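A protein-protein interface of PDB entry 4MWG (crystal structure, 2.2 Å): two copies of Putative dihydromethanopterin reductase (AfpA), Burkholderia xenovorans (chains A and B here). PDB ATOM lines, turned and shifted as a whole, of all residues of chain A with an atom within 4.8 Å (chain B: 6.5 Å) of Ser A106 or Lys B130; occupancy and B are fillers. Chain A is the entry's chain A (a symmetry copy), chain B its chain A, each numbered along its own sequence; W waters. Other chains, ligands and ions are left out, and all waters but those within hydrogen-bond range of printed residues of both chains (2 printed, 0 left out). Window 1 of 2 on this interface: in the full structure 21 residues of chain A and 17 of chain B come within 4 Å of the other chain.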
ATOM      1  N   ALA A 104      -6.297 -10.220 -28.012  1.00  0.00           N
ATOM      2  CA  ALA A 104      -6.289  -8.945 -27.294  1.00  0.00           C
ATOM      3  C   ALA A 104      -7.046  -9.118 -25.983  1.00  0.00           C
ATOM      4  O   ALA A 104      -8.248  -9.379 -25.994  1.00  0.00           O
ATOM      5  CB  ALA A 104      -6.922  -7.836 -28.143  1.00  0.00           C
ATOM      6  N   THR A 105      -6.337  -9.021 -24.864  1.00  0.00           N
ATOM      7  CA  THR A 105      -6.960  -9.056 -23.541  1.00  0.00           C
ATOM      8  C   THR A 105      -7.946  -7.908 -23.355  1.00  0.00           C
ATOM      9  O   THR A 105      -7.886  -6.908 -24.087  1.00  0.00           O
ATOM     10  CB  THR A 105      -5.921  -8.934 -22.434  1.00  0.00           C
ATOM     11  OG1 THR A 105      -5.151  -7.746 -22.677  1.00  0.00           O
ATOM     12  CG2 THR A 105      -5.005 -10.156 -22.396  1.00  0.00           C
ATOM     13  N   SER A 106      -8.846  -8.047 -22.379  1.00  0.00           N
ATOM     14  CA  SER A 106      -9.767  -6.974 -22.048  1.00  0.00           C
ATOM     15  C   SER A 106      -8.961  -5.753 -21.596  1.00  0.00           C
ATOM     16  O   SER A 106      -9.313  -4.608 -21.889  1.00  0.00           O
ATOM     17  CB  SER A 106     -10.747  -7.422 -20.962  1.00  0.00           C
ATOM     18  OG  SER A 106     -10.043  -7.959 -19.852  1.00  0.00           O
ATOM     19  N   ASN A 107      -7.864  -6.005 -20.894  1.00  0.00           N
ATOM     20  CA  ASN A 107      -7.013  -4.920 -20.449  1.00  0.00           C
ATOM     21  C   ASN A 107      -6.497  -4.081 -21.636  1.00  0.00           C
ATOM     22  O   ASN A 107      -6.513  -2.853 -21.586  1.00  0.00           O
ATOM     23  CB  ASN A 107      -5.838  -5.465 -19.626  1.00  0.00           C
ATOM     24  CG  ASN A 107      -4.814  -4.401 -19.321  1.00  0.00           C
ATOM     25  OD1 ASN A 107      -5.067  -3.487 -18.515  1.00  0.00           O
ATOM     26  ND2 ASN A 107      -3.643  -4.498 -19.970  1.00  0.00           N
ATOM     27  N   THR A 108      -6.047  -4.748 -22.699  1.00  0.00           N
ATOM     28  CA  THR A 108      -5.532  -4.045 -23.882  1.00  0.00           C
ATOM     29  C   THR A 108      -6.673  -3.366 -24.669  1.00  0.00           C
ATOM     30  O   THR A 108      -6.538  -2.228 -25.124  1.00  0.00           O
ATOM     31  CB  THR A 108      -4.728  -5.013 -24.800  1.00  0.00           C
ATOM     32  OG1 THR A 108      -3.423  -5.227 -24.230  1.00  0.00           O
ATOM     33  CG2 THR A 108      -4.556  -4.423 -26.219  1.00  0.00           C
ATOM     34  N   VAL A 109      -7.811  -4.041 -24.794  1.00  0.00           N
ATOM     35  CA  VAL A 109      -8.967  -3.418 -25.441  1.00  0.00           C
ATOM     36  C   VAL A 109      -9.362  -2.117 -24.700  1.00  0.00           C
ATOM     37  O   VAL A 109      -9.657  -1.096 -25.321  1.00  0.00           O
ATOM     38  CB  VAL A 109     -10.158  -4.389 -25.492  1.00  0.00           C
ATOM     39  CG1 VAL A 109     -11.430  -3.643 -25.883  1.00  0.00           C
ATOM     40  CG2 VAL A 109      -9.846  -5.567 -26.454  1.00  0.00           C
ATOM     41  N   ALA A 110      -9.322  -2.163 -23.370  1.00  0.00           N
ATOM     42  CA  ALA A 110      -9.625  -1.009 -22.534  1.00  0.00           C
ATOM     43  C   ALA A 110      -8.669   0.137 -22.829  1.00  0.00           C
ATOM     44  O   ALA A 110      -9.100   1.262 -23.103  1.00  0.00           O
ATOM     45  CB  ALA A 110      -9.539  -1.381 -21.048  1.00  0.00           C
ATOM     46  N   ASP A 141     -12.037 -12.035 -25.364  1.00  0.00           N
ATOM     47  CA  ASP A 141     -12.832 -12.235 -24.152  1.00  0.00           C
ATOM     48  C   ASP A 141     -14.165 -11.484 -24.191  1.00  0.00           C
ATOM     49  O   ASP A 141     -14.423 -10.651 -23.329  1.00  0.00           O
ATOM     50  CB  ASP A 141     -12.024 -11.805 -22.911  1.00  0.00           C
ATOM     51  CG  ASP A 141     -10.731 -12.612 -22.729  1.00  0.00           C
ATOM     52  OD1 ASP A 141     -10.726 -13.819 -23.056  1.00  0.00           O
ATOM     53  OD2 ASP A 141      -9.720 -12.043 -22.258  1.00  0.00           O
ATOM     54  N   GLU A 156     -17.018 -21.047 -15.456  1.00  0.00           N
ATOM     55  CA  GLU A 156     -17.538 -20.148 -16.475  1.00  0.00           C
ATOM     56  C   GLU A 156     -17.076 -18.705 -16.285  1.00  0.00           C
ATOM     57  O   GLU A 156     -17.300 -18.113 -15.234  1.00  0.00           O
ATOM     58  CB  GLU A 156     -19.066 -20.197 -16.478  1.00  0.00           C
ATOM     59  CG  GLU A 156     -19.680 -19.320 -17.543  1.00  0.00           C
ATOM     60  CD  GLU A 156     -21.175 -19.495 -17.644  1.00  0.00           C
ATOM     61  OE1 GLU A 156     -21.776 -18.833 -18.508  1.00  0.00           O
ATOM     62  OE2 GLU A 156     -21.743 -20.284 -16.862  1.00  0.00           O
ATOM     63  N   LEU A 157     -16.443 -18.141 -17.306  1.00  0.00           N
ATOM     64  CA  LEU A 157     -16.139 -16.719 -17.319  1.00  0.00           C
ATOM     65  C   LEU A 157     -17.121 -15.960 -18.206  1.00  0.00           C
ATOM     66  O   LEU A 157     -17.391 -16.380 -19.328  1.00  0.00           O
ATOM     67  CB  LEU A 157     -14.722 -16.463 -17.812  1.00  0.00           C
ATOM     68  CG  LEU A 157     -13.556 -17.176 -17.130  1.00  0.00           C
ATOM     69  CD1 LEU A 157     -12.263 -16.487 -17.536  1.00  0.00           C
ATOM     70  CD2 LEU A 157     -13.723 -17.177 -15.633  1.00  0.00           C
ATOM     71  N   ARG A 158     -17.641 -14.843 -17.699  1.00  0.00           N
ATOM     72  CA  ARG A 158     -18.584 -14.001 -18.441  1.00  0.00           C
ATOM     73  C   ARG A 158     -18.096 -12.557 -18.482  1.00  0.00           C
ATOM     74  O   ARG A 158     -17.781 -11.982 -17.448  1.00  0.00           O
ATOM     75  CB  ARG A 158     -19.976 -14.064 -17.811  1.00  0.00           C
ATOM     76  CG  ARG A 158     -20.509 -15.484 -17.657  1.00  0.00           C
ATOM     77  CD  ARG A 158     -21.897 -15.506 -17.023  1.00  0.00           C
ATOM     78  NE  ARG A 158     -22.902 -14.881 -17.882  1.00  0.00           N
ATOM     79  CZ  ARG A 158     -23.742 -15.547 -18.672  1.00  0.00           C
ATOM     80  NH1 ARG A 158     -23.710 -16.873 -18.717  1.00  0.00           N
ATOM     81  NH2 ARG A 158     -24.619 -14.887 -19.419  1.00  0.00           N
ATOM     82  N   ARG A 160     -17.997  -8.638 -18.347  1.00  0.00           N
ATOM     83  CA  ARG A 160     -18.861  -7.699 -17.641  1.00  0.00           C
ATOM     84  C   ARG A 160     -19.306  -6.607 -18.617  1.00  0.00           C
ATOM     85  O   ARG A 160     -18.811  -6.535 -19.751  1.00  0.00           O
ATOM     86  CB  ARG A 160     -18.136  -7.103 -16.420  1.00  0.00           C
ATOM     87  CG  ARG A 160     -17.637  -8.150 -15.407  1.00  0.00           C
ATOM     88  CD  ARG A 160     -16.531  -7.587 -14.487  1.00  0.00           C
ATOM     89  NE  ARG A 160     -15.416  -7.070 -15.267  1.00  0.00           N
ATOM     90  CZ  ARG A 160     -14.477  -6.243 -14.807  1.00  0.00           C
ATOM     91  NH1 ARG A 160     -14.474  -5.832 -13.546  1.00  0.00           N
ATOM     92  NH2 ARG A 160     -13.527  -5.836 -15.616  1.00  0.00           N
ATOM     93  N   GLU A 163     -16.384  -4.689 -20.191  1.00  0.00           N
ATOM     94  CA  GLU A 163     -15.758  -5.361 -21.332  1.00  0.00           C
ATOM     95  C   GLU A 163     -16.567  -5.123 -22.617  1.00  0.00           C
ATOM     96  O   GLU A 163     -15.996  -4.927 -23.685  1.00  0.00           O
ATOM     97  CB  GLU A 163     -15.629  -6.873 -21.086  1.00  0.00           C
ATOM     98  CG  GLU A 163     -14.394  -7.322 -20.316  1.00  0.00           C
ATOM     99  CD  GLU A 163     -14.521  -7.093 -18.824  1.00  0.00           C
ATOM    100  OE1 GLU A 163     -15.524  -7.541 -18.225  1.00  0.00           O
ATOM    101  OE2 GLU A 163     -13.617  -6.455 -18.250  1.00  0.00           O
ATOM    102  N   PHE B 114     -12.617   1.506 -15.415  1.00  0.00           N
ATOM    103  CA  PHE B 114     -12.561   1.506 -16.870  1.00  0.00           C
ATOM    104  C   PHE B 114     -12.146   0.147 -17.431  1.00  0.00           C
ATOM    105  O   PHE B 114     -11.976  -0.009 -18.641  1.00  0.00           O
ATOM    106  CB  PHE B 114     -11.645   2.638 -17.353  1.00  0.00           C
ATOM    107  CG  PHE B 114     -12.248   4.004 -17.138  1.00  0.00           C
ATOM    108  CD1 PHE B 114     -13.332   4.420 -17.901  1.00  0.00           C
ATOM    109  CD2 PHE B 114     -11.769   4.849 -16.153  1.00  0.00           C
ATOM    110  CE1 PHE B 114     -13.914   5.662 -17.691  1.00  0.00           C
ATOM    111  CE2 PHE B 114     -12.342   6.093 -15.942  1.00  0.00           C
ATOM    112  CZ  PHE B 114     -13.406   6.502 -16.708  1.00  0.00           C
ATOM    113  N   GLY B 115     -12.049  -0.849 -16.550  1.00  0.00           N
ATOM    114  CA  GLY B 115     -11.769  -2.206 -16.980  1.00  0.00           C
ATOM    115  C   GLY B 115     -10.302  -2.445 -17.303  1.00  0.00           C
ATOM    116  O   GLY B 115      -9.966  -3.371 -18.045  1.00  0.00           O
ATOM    117  N   ILE B 116      -9.427  -1.610 -16.751  1.00  0.00           N
ATOM    118  CA  ILE B 116      -7.988  -1.777 -16.928  1.00  0.00           C
ATOM    119  C   ILE B 116      -7.491  -2.683 -15.813  1.00  0.00           C
ATOM    120  O   ILE B 116      -7.883  -2.516 -14.655  1.00  0.00           O
ATOM    121  CB  ILE B 116      -7.218  -0.418 -16.886  1.00  0.00           C
ATOM    122  CG1 ILE B 116      -7.452   0.351 -18.175  1.00  0.00           C
ATOM    123  CG2 ILE B 116      -5.703  -0.645 -16.646  1.00  0.00           C
ATOM    124  CD1 ILE B 116      -7.157   1.823 -18.089  1.00  0.00           C
ATOM    125  N   SER B 117      -6.650  -3.655 -16.145  1.00  0.00           N
ATOM    126  CA  SER B 117      -6.141  -4.557 -15.117  1.00  0.00           C
ATOM    127  C   SER B 117      -4.644  -4.845 -15.324  1.00  0.00           C
ATOM    128  O   SER B 117      -4.276  -5.925 -15.761  1.00  0.00           O
ATOM    129  CB  SER B 117      -6.948  -5.860 -15.120  1.00  0.00           C
ATOM    130  OG  SER B 117      -6.940  -6.457 -16.406  1.00  0.00           O
ATOM    131  N   TYR B 125      -9.580  -7.997  -9.117  1.00  0.00           N
ATOM    132  CA  TYR B 125     -10.934  -7.472  -9.160  1.00  0.00           C
ATOM    133  C   TYR B 125     -11.650  -7.826 -10.476  1.00  0.00           C
ATOM    134  O   TYR B 125     -12.789  -8.282 -10.456  1.00  0.00           O
ATOM    135  CB  TYR B 125     -10.929  -5.949  -8.936  1.00  0.00           C
ATOM    136  CG  TYR B 125     -12.290  -5.350  -9.180  1.00  0.00           C
ATOM    137  CD1 TYR B 125     -13.292  -5.435  -8.214  1.00  0.00           C
ATOM    138  CD2 TYR B 125     -12.595  -4.737 -10.395  1.00  0.00           C
ATOM    139  CE1 TYR B 125     -14.558  -4.908  -8.442  1.00  0.00           C
ATOM    140  CE2 TYR B 125     -13.847  -4.204 -10.633  1.00  0.00           C
ATOM    141  CZ  TYR B 125     -14.827  -4.287  -9.649  1.00  0.00           C
ATOM    142  OH  TYR B 125     -16.084  -3.773  -9.894  1.00  0.00           O
ATOM    143  N   ALA B 126     -10.985  -7.649 -11.622  1.00  0.00           N
ATOM    144  CA  ALA B 126     -11.612  -7.967 -12.905  1.00  0.00           C
ATOM    145  C   ALA B 126     -11.905  -9.466 -13.099  1.00  0.00           C
ATOM    146  O   ALA B 126     -12.965  -9.835 -13.620  1.00  0.00           O
ATOM    147  CB  ALA B 126     -10.748  -7.454 -14.067  1.00  0.00           C
ATOM    148  N   GLN B 127     -10.974 -10.331 -12.720  1.00  0.00           N
ATOM    149  CA  GLN B 127     -11.218 -11.770 -12.879  1.00  0.00           C
ATOM    150  C   GLN B 127     -12.330 -12.245 -11.935  1.00  0.00           C
ATOM    151  O   GLN B 127     -13.115 -13.111 -12.295  1.00  0.00           O
ATOM    152  CB  GLN B 127      -9.947 -12.586 -12.632  1.00  0.00           C
ATOM    153  CG  GLN B 127      -8.904 -12.447 -13.724  1.00  0.00           C
ATOM    154  CD  GLN B 127      -9.357 -13.057 -15.027  1.00  0.00           C
ATOM    155  OE1 GLN B 127      -9.814 -14.199 -15.058  1.00  0.00           O
ATOM    156  NE2 GLN B 127      -9.252 -12.294 -16.114  1.00  0.00           N
ATOM    157  N   ALA B 128     -12.383 -11.681 -10.732  1.00  0.00           N
ATOM    158  CA  ALA B 128     -13.463 -11.993  -9.795  1.00  0.00           C
ATOM    159  C   ALA B 128     -14.818 -11.684 -10.421  1.00  0.00           C
ATOM    160  O   ALA B 128     -15.711 -12.530 -10.450  1.00  0.00           O
ATOM    161  CB  ALA B 128     -13.297 -11.216  -8.502  1.00  0.00           C
ATOM    162  N   GLY B 129     -14.954 -10.467 -10.936  1.00  0.00           N
ATOM    163  CA  GLY B 129     -16.182 -10.058 -11.596  1.00  0.00           C
ATOM    164  C   GLY B 129     -16.582 -10.933 -12.759  1.00  0.00           C
ATOM    165  O   GLY B 129     -17.769 -11.183 -12.966  1.00  0.00           O
ATOM    166  N   LYS B 130     -15.609 -11.411 -13.524  1.00  0.00           N
ATOM    167  CA  LYS B 130     -15.925 -12.269 -14.672  1.00  0.00           C
ATOM    168  C   LYS B 130     -16.422 -13.631 -14.197  1.00  0.00           C
ATOM    169  O   LYS B 130     -17.136 -14.319 -14.923  1.00  0.00           O
ATOM    170  CB  LYS B 130     -14.709 -12.442 -15.591  1.00  0.00           C
ATOM    171  CG  LYS B 130     -14.200 -11.149 -16.224  1.00  0.00           C
ATOM    172  CD  LYS B 130     -12.964 -11.391 -17.094  1.00  0.00           C
ATOM    173  CE  LYS B 130     -12.353 -10.076 -17.595  1.00  0.00           C
ATOM    174  NZ  LYS B 130     -11.338 -10.285 -18.675  1.00  0.00           N
ATOM    175  N   GLN B 131     -16.047 -14.013 -12.976  1.00  0.00           N
ATOM    176  CA  GLN B 131     -16.533 -15.266 -12.383  1.00  0.00           C
ATOM    177  C   GLN B 131     -17.721 -15.051 -11.452  1.00  0.00           C
ATOM    178  O   GLN B 131     -18.123 -15.968 -10.743  1.00  0.00           O
ATOM    179  CB  GLN B 131     -15.424 -15.960 -11.594  1.00  0.00           C
ATOM    180  CG  GLN B 131     -14.166 -16.195 -12.376  1.00  0.00           C
ATOM    181  CD  GLN B 131     -13.107 -16.939 -11.586  1.00  0.00           C
ATOM    182  OE1 GLN B 131     -11.953 -16.517 -11.534  1.00  0.00           O
ATOM    183  NE2 GLN B 131     -13.490 -18.061 -10.979  1.00  0.00           N
ATOM    184  N   CYS B 132     -18.244 -13.826 -11.423  1.00  0.00           N
ATOM    185  CA  CYS B 132     -19.349 -13.460 -10.535  1.00  0.00           C
ATOM    186  C   CYS B 132     -19.002 -13.636  -9.052  1.00  0.00           C
ATOM    187  O   CYS B 132     -19.874 -13.904  -8.234  1.00  0.00           O
ATOM    188  CB  CYS B 132     -20.604 -14.276 -10.876  1.00  0.00           C
ATOM    189  SG  CYS B 132     -21.074 -14.188 -12.614  1.00  0.00           S
ATOM    190  N   ILE B 133     -17.724 -13.485  -8.720  1.00  0.00           N
ATOM    191  CA  ILE B 133     -17.271 -13.421  -7.337  1.00  0.00           C
ATOM    192  C   ILE B 133     -17.349 -11.974  -6.836  1.00  0.00           C
ATOM    193  O   ILE B 133     -16.792 -11.074  -7.460  1.00  0.00           O
ATOM    194  CB  ILE B 133     -15.824 -13.936  -7.195  1.00  0.00           C
ATOM    195  CG1 ILE B 133     -15.729 -15.415  -7.609  1.00  0.00           C
ATOM    196  CG2 ILE B 133     -15.289 -13.698  -5.771  1.00  0.00           C
ATOM    197  CD1 ILE B 133     -14.294 -15.893  -7.701  1.00  0.00           C
ATOM    198  N   TYR B 175     -21.954  -7.179  -9.007  1.00  0.00           N
ATOM    199  CA  TYR B 175     -21.183  -7.930  -8.014  1.00  0.00           C
ATOM    200  C   TYR B 175     -20.205  -7.061  -7.238  1.00  0.00           C
ATOM    201  O   TYR B 175     -19.209  -7.555  -6.705  1.00  0.00           O
ATOM    202  CB  TYR B 175     -20.421  -9.082  -8.689  1.00  0.00           C
ATOM    203  CG  TYR B 175     -21.322  -9.982  -9.502  1.00  0.00           C
ATOM    204  CD1 TYR B 175     -22.345 -10.689  -8.891  1.00  0.00           C
ATOM    205  CD2 TYR B 175     -21.156 -10.109 -10.875  1.00  0.00           C
ATOM    206  CE1 TYR B 175     -23.186 -11.504  -9.623  1.00  0.00           C
ATOM    207  CE2 TYR B 175     -21.989 -10.921 -11.617  1.00  0.00           C
ATOM    208  CZ  TYR B 175     -23.002 -11.617 -10.984  1.00  0.00           C
ATOM    209  OH  TYR B 175     -23.839 -12.429 -11.710  1.00  0.00           O
HETATM  210  O   HOH W   1     -12.158  -4.539 -19.314  1.00  0.00           O
HETATM  211  O   HOH W   2      -9.298  -5.984 -17.950  1.00  0.00           O
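The backbone NH (N) of Ser B117 is in hydrogen-bond range of the side-chain amide oxygen (OD1) of Asn A107 (2.9 Å).
OG of Ser A106 lies within hydrogen-bond range of NZ of Lys B130 (2.9 Å).
The backbone carbonyl oxygen (O) of Lys B130 sits at hydrogen-bond distance from the backbone NH (N) of Arg A158, at 2.9 Å.
OE1 of Glu A156 lies within salt-bridge range of NH1 of Arg A158.
The guanidinium group (NH2) of Arg A160 lies within salt-bridge range of the side-chain carboxylate (OE2) of Glu A163 (2.7 Å).
Among the printed residues, pairs that only touch across the chains: Arg A160 with Tyr B125, Leu A157 with Gln B131, Asn A107 with Ile B116, Leu A157 with Lys B130, Arg A160 with Ala B126, Ala A110 with Gly B115, Ala A110 with Phe B114, Arg A160 with Gly B129, Glu A156 with Lys B130, Glu A163 with Lys B130 and Ala A110 with Ile B116.
Ala A104 touches none of the printed residues of chain B.
Of the printed residues of chain B, Asn A107 touches Ile B116 (3.5 Å) and Ser B117 (2.9 Å).
Of the printed residues of chain B, Ala A110 touches Phe B114, Gly B115 and Ile B116.
Printed residues of chain B within 4 Å of Leu A157: Lys B130 (3.5 Å) and Gln B131 (3.4 Å).
Of the printed residues of chain A, Gly B115 touches Ala A110.
Printed residues of chain A within 4 Å of Ala B126: Arg A160 (3.6 Å).
Cys B132 touches none of the printed residues of chain A.
The nearest printed residue of chain B that does not touch Ser A106 is Gly B115 (4.1 Å).
Hydrophobic or aromatic side chains of chain A within 4 Å of the printed part of chain B: Ala A110 and Leu A157.
Among the printed residues, no Asp or Glu carboxylate lies within 4 Å of a Lys or Arg side-chain nitrogen of the other chain.
No position is printed for both chains.
Of the 14 pairs that touch across the chains among the printed residues, none has its exchanged pair printed and touching as well.
Water W1 lies within hydrogen-bond range of the side-chain carboxylate (OE2) of Glu A163 and the backbone carbonyl oxygen (O) of Gly B115.
Water W2 lies within hydrogen-bond range of O of Gly B115, OG of Ser A106, OG of Ser B117 and N of Asn A107.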
